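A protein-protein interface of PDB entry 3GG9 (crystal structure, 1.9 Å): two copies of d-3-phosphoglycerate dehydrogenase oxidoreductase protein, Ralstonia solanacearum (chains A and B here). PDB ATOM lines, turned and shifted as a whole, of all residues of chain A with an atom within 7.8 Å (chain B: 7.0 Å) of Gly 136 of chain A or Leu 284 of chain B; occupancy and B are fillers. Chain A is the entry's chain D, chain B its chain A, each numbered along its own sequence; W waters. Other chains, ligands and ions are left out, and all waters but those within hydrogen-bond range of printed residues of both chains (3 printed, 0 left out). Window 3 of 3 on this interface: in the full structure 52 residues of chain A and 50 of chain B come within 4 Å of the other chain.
The backbone carbonyl oxygen of Tyr 11 of chain B is in hydrogen-bond range of the side-chain amide nitrogen of Gln 140 of chain A, at 3.0 Å. The backbone carbonyl oxygen (O) of Leu 290 of chain B lies within hydrogen-bond range of the side-chain amino group (NZ) of Lys 134 of chain A (2.9 Å).
The side-chain hydroxyl (OG) of Ser 132 of chain A sits at hydrogen-bond distance from the backbone carbonyl oxygen (O) of Gln 140 of chain A (2.9 Å). OG1 of Thr 35 of chain B lies within hydrogen-bond range of OH of Tyr 11 of chain B, 2.6 Å away.
CD1 of Leu 133 of chain A touches O of Ile 283 of chain B (3.8 Å). O of Leu 133 of chain A touches CD1 of Leu 290 of chain B (3.7 Å). Leu 284 of chain B touches Gly 136 of chain A. Trp 138 of chain A touches Tyr 11 of chain B. Trp 138 of chain A touches Glu 281 of chain B (CH2 to CG, 3.7 Å). Trp 138 of chain A touches Pro 282 of chain B. CE3 of Trp 138 of chain A touches N of Ile 283 of chain B, at 3.3 Å. Leu 284 of chain B touches Trp 138 of chain A. Gln 139 of chain A touches Tyr 11 of chain B.
Gly 136 of chain A touches one residue of chain B. Printed residues of chain B within 4 Å of Gln 139 of chain A: Tyr 11 (3.3 Å). Printed residues of chain A within 4 Å of Tyr 11 of chain B: Trp 138, Gln 139 and Gln 140. Thr 35 of chain B touches none of the printed residues of chain A. Printed residues of chain A within 4 Å of Glu 281 of chain B: Trp 138 (3.7 Å). Of chain A, only Gly 136 and Trp 138 come within 4 Å of Leu 284 of chain B. Printed residues of chain A within 4 Å of Leu 290 of chain B: Leu 133 and Lys 134. The nearest residue of chain B that does not touch Gly 136 of chain A is Ile 283 of chain B (4.6 Å). The nearest residue of chain A that does not touch Leu 284 of chain B is Ala 137 of chain A (5.1 Å).
Of the 11 printed residues of chain A, 6 touch a printed residue of chain B. Hydrophobic or aromatic side chains of chain A within 4 Å of the printed part of chain B: Leu 133 and Trp 138. Along chain B the printed residues that touch a printed residue of chain A span positions 11 to 290. Among the printed residues, no Asp or Glu carboxylate lies within 4 Å of a Lys or Arg side-chain nitrogen of the other chain.
No position is printed for both chains. Of the 11 pairs that touch across the chains among the printed residues, none has its exchanged pair printed and touching as well.
Water W1 lies within hydrogen-bond range of the backbone carbonyl oxygen of Gly 136 of chain A (2.6 Å) and the backbone carbonyl oxygen of Leu 284 of chain B (2.7 Å). Water W3 lies within hydrogen-bond range of O of Leu 290 of chain B and NZ of Lys 134 of chain A. Water W2 lies within hydrogen-bond range of the indole nitrogen (NE1) of Trp 138 of chain A (3.3 Å) and the side-chain carboxylate (OE1) of Glu 281 of chain B (3.4 Å).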
ATOM      1  N   VAL A 130     -26.151  17.791   8.176  1.00  0.00           N
ATOM      2  CA  VAL A 130     -24.956  17.604   9.027  1.00  0.00           C
ATOM      3  C   VAL A 130     -25.237  17.946  10.498  1.00  0.00           C
ATOM      4  O   VAL A 130     -24.884  17.179  11.385  1.00  0.00           O
ATOM      5  CB  VAL A 130     -23.735  18.426   8.460  1.00  0.00           C
ATOM      6  CG1 VAL A 130     -22.602  18.563   9.472  1.00  0.00           C
ATOM      7  CG2 VAL A 130     -23.200  17.789   7.189  1.00  0.00           C
ATOM      8  N   ALA A 131     -25.879  19.089  10.729  1.00  0.00           N
ATOM      9  CA  ALA A 131     -26.163  19.581  12.075  1.00  0.00           C
ATOM     10  C   ALA A 131     -27.180  18.706  12.774  1.00  0.00           C
ATOM     11  O   ALA A 131     -27.047  18.434  13.967  1.00  0.00           O
ATOM     12  CB  ALA A 131     -26.647  21.029  12.022  1.00  0.00           C
ATOM     13  N   SER A 132     -28.181  18.256  12.020  1.00  0.00           N
ATOM     14  CA  SER A 132     -29.209  17.369  12.536  1.00  0.00           C
ATOM     15  C   SER A 132     -28.617  16.034  12.947  1.00  0.00           C
ATOM     16  O   SER A 132     -28.945  15.525  14.027  1.00  0.00           O
ATOM     17  CB  SER A 132     -30.268  17.115  11.477  1.00  0.00           C
ATOM     18  OG  SER A 132     -30.886  18.331  11.114  1.00  0.00           O
ATOM     19  N   LEU A 133     -27.737  15.485  12.099  1.00  0.00           N
ATOM     20  CA  LEU A 133     -27.098  14.195  12.381  1.00  0.00           C
ATOM     21  C   LEU A 133     -26.277  14.291  13.666  1.00  0.00           C
ATOM     22  O   LEU A 133     -26.364  13.397  14.517  1.00  0.00           O
ATOM     23  CB  LEU A 133     -26.252  13.664  11.197  1.00  0.00           C
ATOM     24  CG  LEU A 133     -25.434  12.361  11.417  1.00  0.00           C
ATOM     25  CD1 LEU A 133     -26.217  11.152  11.956  1.00  0.00           C
ATOM     26  CD2 LEU A 133     -24.667  11.931  10.182  1.00  0.00           C
ATOM     27  N   LYS A 134     -25.526  15.383  13.805  1.00  0.00           N
ATOM     28  CA  LYS A 134     -24.731  15.664  15.018  1.00  0.00           C
ATOM     29  C   LYS A 134     -25.607  15.729  16.278  1.00  0.00           C
ATOM     30  O   LYS A 134     -25.148  15.406  17.370  1.00  0.00           O
ATOM     31  CB  LYS A 134     -23.953  16.967  14.879  1.00  0.00           C
ATOM     32  CG  LYS A 134     -22.626  16.852  14.147  1.00  0.00           C
ATOM     33  CD  LYS A 134     -21.968  18.214  14.055  1.00  0.00           C
ATOM     34  CE  LYS A 134     -20.582  18.133  13.471  1.00  0.00           C
ATOM     35  NZ  LYS A 134     -19.543  17.739  14.470  1.00  0.00           N
ATOM     36  N   HIS A 135     -26.859  16.140  16.109  1.00  0.00           N
ATOM     37  CA  HIS A 135     -27.809  16.247  17.220  1.00  0.00           C
ATOM     38  C   HIS A 135     -28.655  14.986  17.407  1.00  0.00           C
ATOM     39  O   HIS A 135     -29.574  14.959  18.219  1.00  0.00           O
ATOM     40  CB  HIS A 135     -28.696  17.496  17.058  1.00  0.00           C
ATOM     41  CG  HIS A 135     -27.998  18.775  17.406  1.00  0.00           C
ATOM     42  ND1 HIS A 135     -27.517  19.648  16.451  1.00  0.00           N
ATOM     43  CD2 HIS A 135     -27.675  19.316  18.606  1.00  0.00           C
ATOM     44  CE1 HIS A 135     -26.944  20.679  17.047  1.00  0.00           C
ATOM     45  NE2 HIS A 135     -27.026  20.502  18.355  1.00  0.00           N
ATOM     46  N   GLY A 136     -28.353  13.948  16.639  1.00  0.00           N
ATOM     47  CA  GLY A 136     -29.017  12.664  16.805  1.00  0.00           C
ATOM     48  C   GLY A 136     -30.221  12.407  15.929  1.00  0.00           C
ATOM     49  O   GLY A 136     -30.954  11.449  16.162  1.00  0.00           O
ATOM     50  N   ALA A 137     -30.441  13.256  14.927  1.00  0.00           N
ATOM     51  CA  ALA A 137     -31.547  13.049  13.998  1.00  0.00           C
ATOM     52  C   ALA A 137     -31.015  12.470  12.688  1.00  0.00           C
ATOM     53  O   ALA A 137     -30.174  13.077  12.032  1.00  0.00           O
ATOM     54  CB  ALA A 137     -32.316  14.346  13.759  1.00  0.00           C
ATOM     55  N   TRP A 138     -31.491  11.287  12.323  1.00  0.00           N
ATOM     56  CA  TRP A 138     -30.968  10.633  11.155  1.00  0.00           C
ATOM     57  C   TRP A 138     -31.766  11.049   9.942  1.00  0.00           C
ATOM     58  O   TRP A 138     -32.976  10.794   9.854  1.00  0.00           O
ATOM     59  CB  TRP A 138     -31.007   9.122  11.296  1.00  0.00           C
ATOM     60  CG  TRP A 138     -30.540   8.426  10.062  1.00  0.00           C
ATOM     61  CD1 TRP A 138     -31.324   7.889   9.085  1.00  0.00           C
ATOM     62  CD2 TRP A 138     -29.185   8.206   9.659  1.00  0.00           C
ATOM     63  NE1 TRP A 138     -30.550   7.338   8.114  1.00  0.00           N
ATOM     64  CE2 TRP A 138     -29.230   7.511   8.437  1.00  0.00           C
ATOM     65  CE3 TRP A 138     -27.937   8.512  10.219  1.00  0.00           C
ATOM     66  CZ2 TRP A 138     -28.076   7.126   7.749  1.00  0.00           C
ATOM     67  CZ3 TRP A 138     -26.788   8.125   9.537  1.00  0.00           C
ATOM     68  CH2 TRP A 138     -26.870   7.437   8.315  1.00  0.00           C
ATOM     69  N   GLN A 139     -31.065  11.687   9.018  1.00  0.00           N
ATOM     70  CA  GLN A 139     -31.607  12.017   7.699  1.00  0.00           C
ATOM     71  C   GLN A 139     -32.798  12.951   7.836  1.00  0.00           C
ATOM     72  O   GLN A 139     -33.872  12.699   7.303  1.00  0.00           O
ATOM     73  CB  GLN A 139     -31.931  10.745   6.917  1.00  0.00           C
ATOM     74  CG  GLN A 139     -31.751  10.878   5.424  1.00  0.00           C
ATOM     75  CD  GLN A 139     -32.012   9.583   4.700  1.00  0.00           C
ATOM     76  OE1 GLN A 139     -33.153   9.251   4.381  1.00  0.00           O
ATOM     77  NE2 GLN A 139     -30.952   8.848   4.418  1.00  0.00           N
ATOM     78  N   GLN A 140     -32.572  14.031   8.575  1.00  0.00           N
ATOM     79  CA  GLN A 140     -33.532  15.100   8.762  1.00  0.00           C
ATOM     80  C   GLN A 140     -32.801  16.383   8.426  1.00  0.00           C
ATOM     81  O   GLN A 140     -31.726  16.660   8.961  1.00  0.00           O
ATOM     82  CB  GLN A 140     -34.062  15.137  10.202  1.00  0.00           C
ATOM     83  CG  GLN A 140     -34.772  13.854  10.663  1.00  0.00           C
ATOM     84  CD  GLN A 140     -36.090  13.594   9.938  1.00  0.00           C
ATOM     85  OE1 GLN A 140     -36.719  14.512   9.409  1.00  0.00           O
ATOM     86  NE2 GLN A 140     -36.518  12.334   9.921  1.00  0.00           N
ATOM     87  N   TYR B  11     -37.499   8.135   6.180  1.00  0.00           N
ATOM     88  CA  TYR B  11     -37.306   8.947   7.393  1.00  0.00           C
ATOM     89  C   TYR B  11     -37.983  10.306   7.312  1.00  0.00           C
ATOM     90  O   TYR B  11     -38.529  10.773   8.297  1.00  0.00           O
ATOM     91  CB  TYR B  11     -35.811   9.085   7.779  1.00  0.00           C
ATOM     92  CG  TYR B  11     -35.104   7.752   7.825  1.00  0.00           C
ATOM     93  CD1 TYR B  11     -35.209   6.927   8.936  1.00  0.00           C
ATOM     94  CD2 TYR B  11     -34.329   7.311   6.752  1.00  0.00           C
ATOM     95  CE1 TYR B  11     -34.583   5.702   8.970  1.00  0.00           C
ATOM     96  CE2 TYR B  11     -33.691   6.092   6.773  1.00  0.00           C
ATOM     97  CZ  TYR B  11     -33.822   5.286   7.897  1.00  0.00           C
ATOM     98  OH  TYR B  11     -33.215   4.058   7.927  1.00  0.00           O
ATOM     99  N   ASN B  34     -39.558   5.228  10.251  1.00  0.00           N
ATOM    100  CA  ASN B  34     -38.386   4.836  11.010  1.00  0.00           C
ATOM    101  C   ASN B  34     -38.039   3.391  10.741  1.00  0.00           C
ATOM    102  O   ASN B  34     -38.786   2.682  10.063  1.00  0.00           O
ATOM    103  CB  ASN B  34     -38.551   5.125  12.508  1.00  0.00           C
ATOM    104  CG  ASN B  34     -39.804   4.511  13.101  1.00  0.00           C
ATOM    105  OD1 ASN B  34     -40.178   3.390  12.778  1.00  0.00           O
ATOM    106  ND2 ASN B  34     -40.453   5.252  13.997  1.00  0.00           N
ATOM    107  N   THR B  35     -36.897   2.966  11.264  1.00  0.00           N
ATOM    108  CA  THR B  35     -36.360   1.646  10.980  1.00  0.00           C
ATOM    109  C   THR B  35     -36.498   0.796  12.225  1.00  0.00           C
ATOM    110  O   THR B  35     -36.278   1.272  13.335  1.00  0.00           O
ATOM    111  CB  THR B  35     -34.870   1.729  10.562  1.00  0.00           C
ATOM    112  OG1 THR B  35     -34.770   2.560   9.407  1.00  0.00           O
ATOM    113  CG2 THR B  35     -34.302   0.358  10.200  1.00  0.00           C
ATOM    114  N   GLU B 281     -26.500   1.767  10.033  1.00  0.00           N
ATOM    115  CA  GLU B 281     -27.390   2.885   9.765  1.00  0.00           C
ATOM    116  C   GLU B 281     -28.789   2.408  10.173  1.00  0.00           C
ATOM    117  O   GLU B 281     -29.103   1.233   9.991  1.00  0.00           O
ATOM    118  CB  GLU B 281     -27.333   3.274   8.271  1.00  0.00           C
ATOM    119  CG  GLU B 281     -25.979   3.901   7.832  1.00  0.00           C
ATOM    120  CD  GLU B 281     -25.823   4.038   6.315  1.00  0.00           C
ATOM    121  OE1 GLU B 281     -26.811   3.871   5.590  1.00  0.00           O
ATOM    122  OE2 GLU B 281     -24.707   4.312   5.842  1.00  0.00           O
ATOM    123  N   PRO B 282     -29.626   3.290  10.763  1.00  0.00           N
ATOM    124  CA  PRO B 282     -29.384   4.686  11.108  1.00  0.00           C
ATOM    125  C   PRO B 282     -28.488   4.875  12.332  1.00  0.00           C
ATOM    126  O   PRO B 282     -28.359   3.977  13.175  1.00  0.00           O
ATOM    127  CB  PRO B 282     -30.786   5.235  11.380  1.00  0.00           C
ATOM    128  CG  PRO B 282     -31.614   4.086  11.664  1.00  0.00           C
ATOM    129  CD  PRO B 282     -31.001   2.875  11.086  1.00  0.00           C
ATOM    130  N   ILE B 283     -27.850   6.031  12.382  1.00  0.00           N
ATOM    131  CA  ILE B 283     -27.045   6.459  13.520  1.00  0.00           C
ATOM    132  C   ILE B 283     -27.932   7.396  14.353  1.00  0.00           C
ATOM    133  O   ILE B 283     -28.160   8.547  13.960  1.00  0.00           O
ATOM    134  CB  ILE B 283     -25.760   7.204  13.038  1.00  0.00           C
ATOM    135  CG1 ILE B 283     -24.872   6.296  12.167  1.00  0.00           C
ATOM    136  CG2 ILE B 283     -24.971   7.786  14.223  1.00  0.00           C
ATOM    137  CD1 ILE B 283     -23.977   5.365  12.958  1.00  0.00           C
ATOM    138  N   LEU B 284     -28.450   6.892  15.475  1.00  0.00           N
ATOM    139  CA  LEU B 284     -29.385   7.644  16.324  1.00  0.00           C
ATOM    140  C   LEU B 284     -28.771   8.006  17.659  1.00  0.00           C
ATOM    141  O   LEU B 284     -29.300   8.846  18.391  1.00  0.00           O
ATOM    142  CB  LEU B 284     -30.682   6.856  16.554  1.00  0.00           C
ATOM    143  CG  LEU B 284     -31.571   6.507  15.351  1.00  0.00           C
ATOM    144  CD1 LEU B 284     -32.887   5.900  15.818  1.00  0.00           C
ATOM    145  CD2 LEU B 284     -31.828   7.728  14.505  1.00  0.00           C
ATOM    146  N   GLN B 285     -27.646   7.368  17.961  1.00  0.00           N
ATOM    147  CA  GLN B 285     -27.005   7.476  19.260  1.00  0.00           C
ATOM    148  C   GLN B 285     -25.562   7.955  19.144  1.00  0.00           C
ATOM    149  O   GLN B 285     -24.764   7.790  20.069  1.00  0.00           O
ATOM    150  CB  GLN B 285     -27.072   6.129  19.979  1.00  0.00           C
ATOM    151  CG  GLN B 285     -27.954   6.104  21.194  1.00  0.00           C
ATOM    152  CD  GLN B 285     -29.400   6.301  20.858  1.00  0.00           C
ATOM    153  OE1 GLN B 285     -29.966   7.358  21.113  1.00  0.00           O
ATOM    154  NE2 GLN B 285     -30.017   5.280  20.279  1.00  0.00           N
ATOM    155  N   GLY B 286     -25.231   8.549  18.001  1.00  0.00           N
ATOM    156  CA  GLY B 286     -23.924   9.168  17.810  1.00  0.00           C
ATOM    157  C   GLY B 286     -22.904   8.210  17.238  1.00  0.00           C
ATOM    158  O   GLY B 286     -23.196   7.025  17.002  1.00  0.00           O
ATOM    159  N   LEU B 290     -18.626  11.709  14.241  1.00  0.00           N
ATOM    160  CA  LEU B 290     -19.486  12.879  14.403  1.00  0.00           C
ATOM    161  C   LEU B 290     -18.908  13.853  15.415  1.00  0.00           C
ATOM    162  O   LEU B 290     -19.235  15.032  15.393  1.00  0.00           O
ATOM    163  CB  LEU B 290     -20.923  12.478  14.801  1.00  0.00           C
ATOM    164  CG  LEU B 290     -21.760  11.583  13.875  1.00  0.00           C
ATOM    165  CD1 LEU B 290     -23.202  11.455  14.351  1.00  0.00           C
ATOM    166  CD2 LEU B 290     -21.747  12.134  12.489  1.00  0.00           C
HETATM  167  O   HOH W   1     -31.740  10.014  18.246  1.00  0.00           O
HETATM  168  O   HOH W   2     -29.902   5.345   5.529  1.00  0.00           O
HETATM  169  O   HOH W   3     -18.266  15.400  12.354  1.00  0.00           O
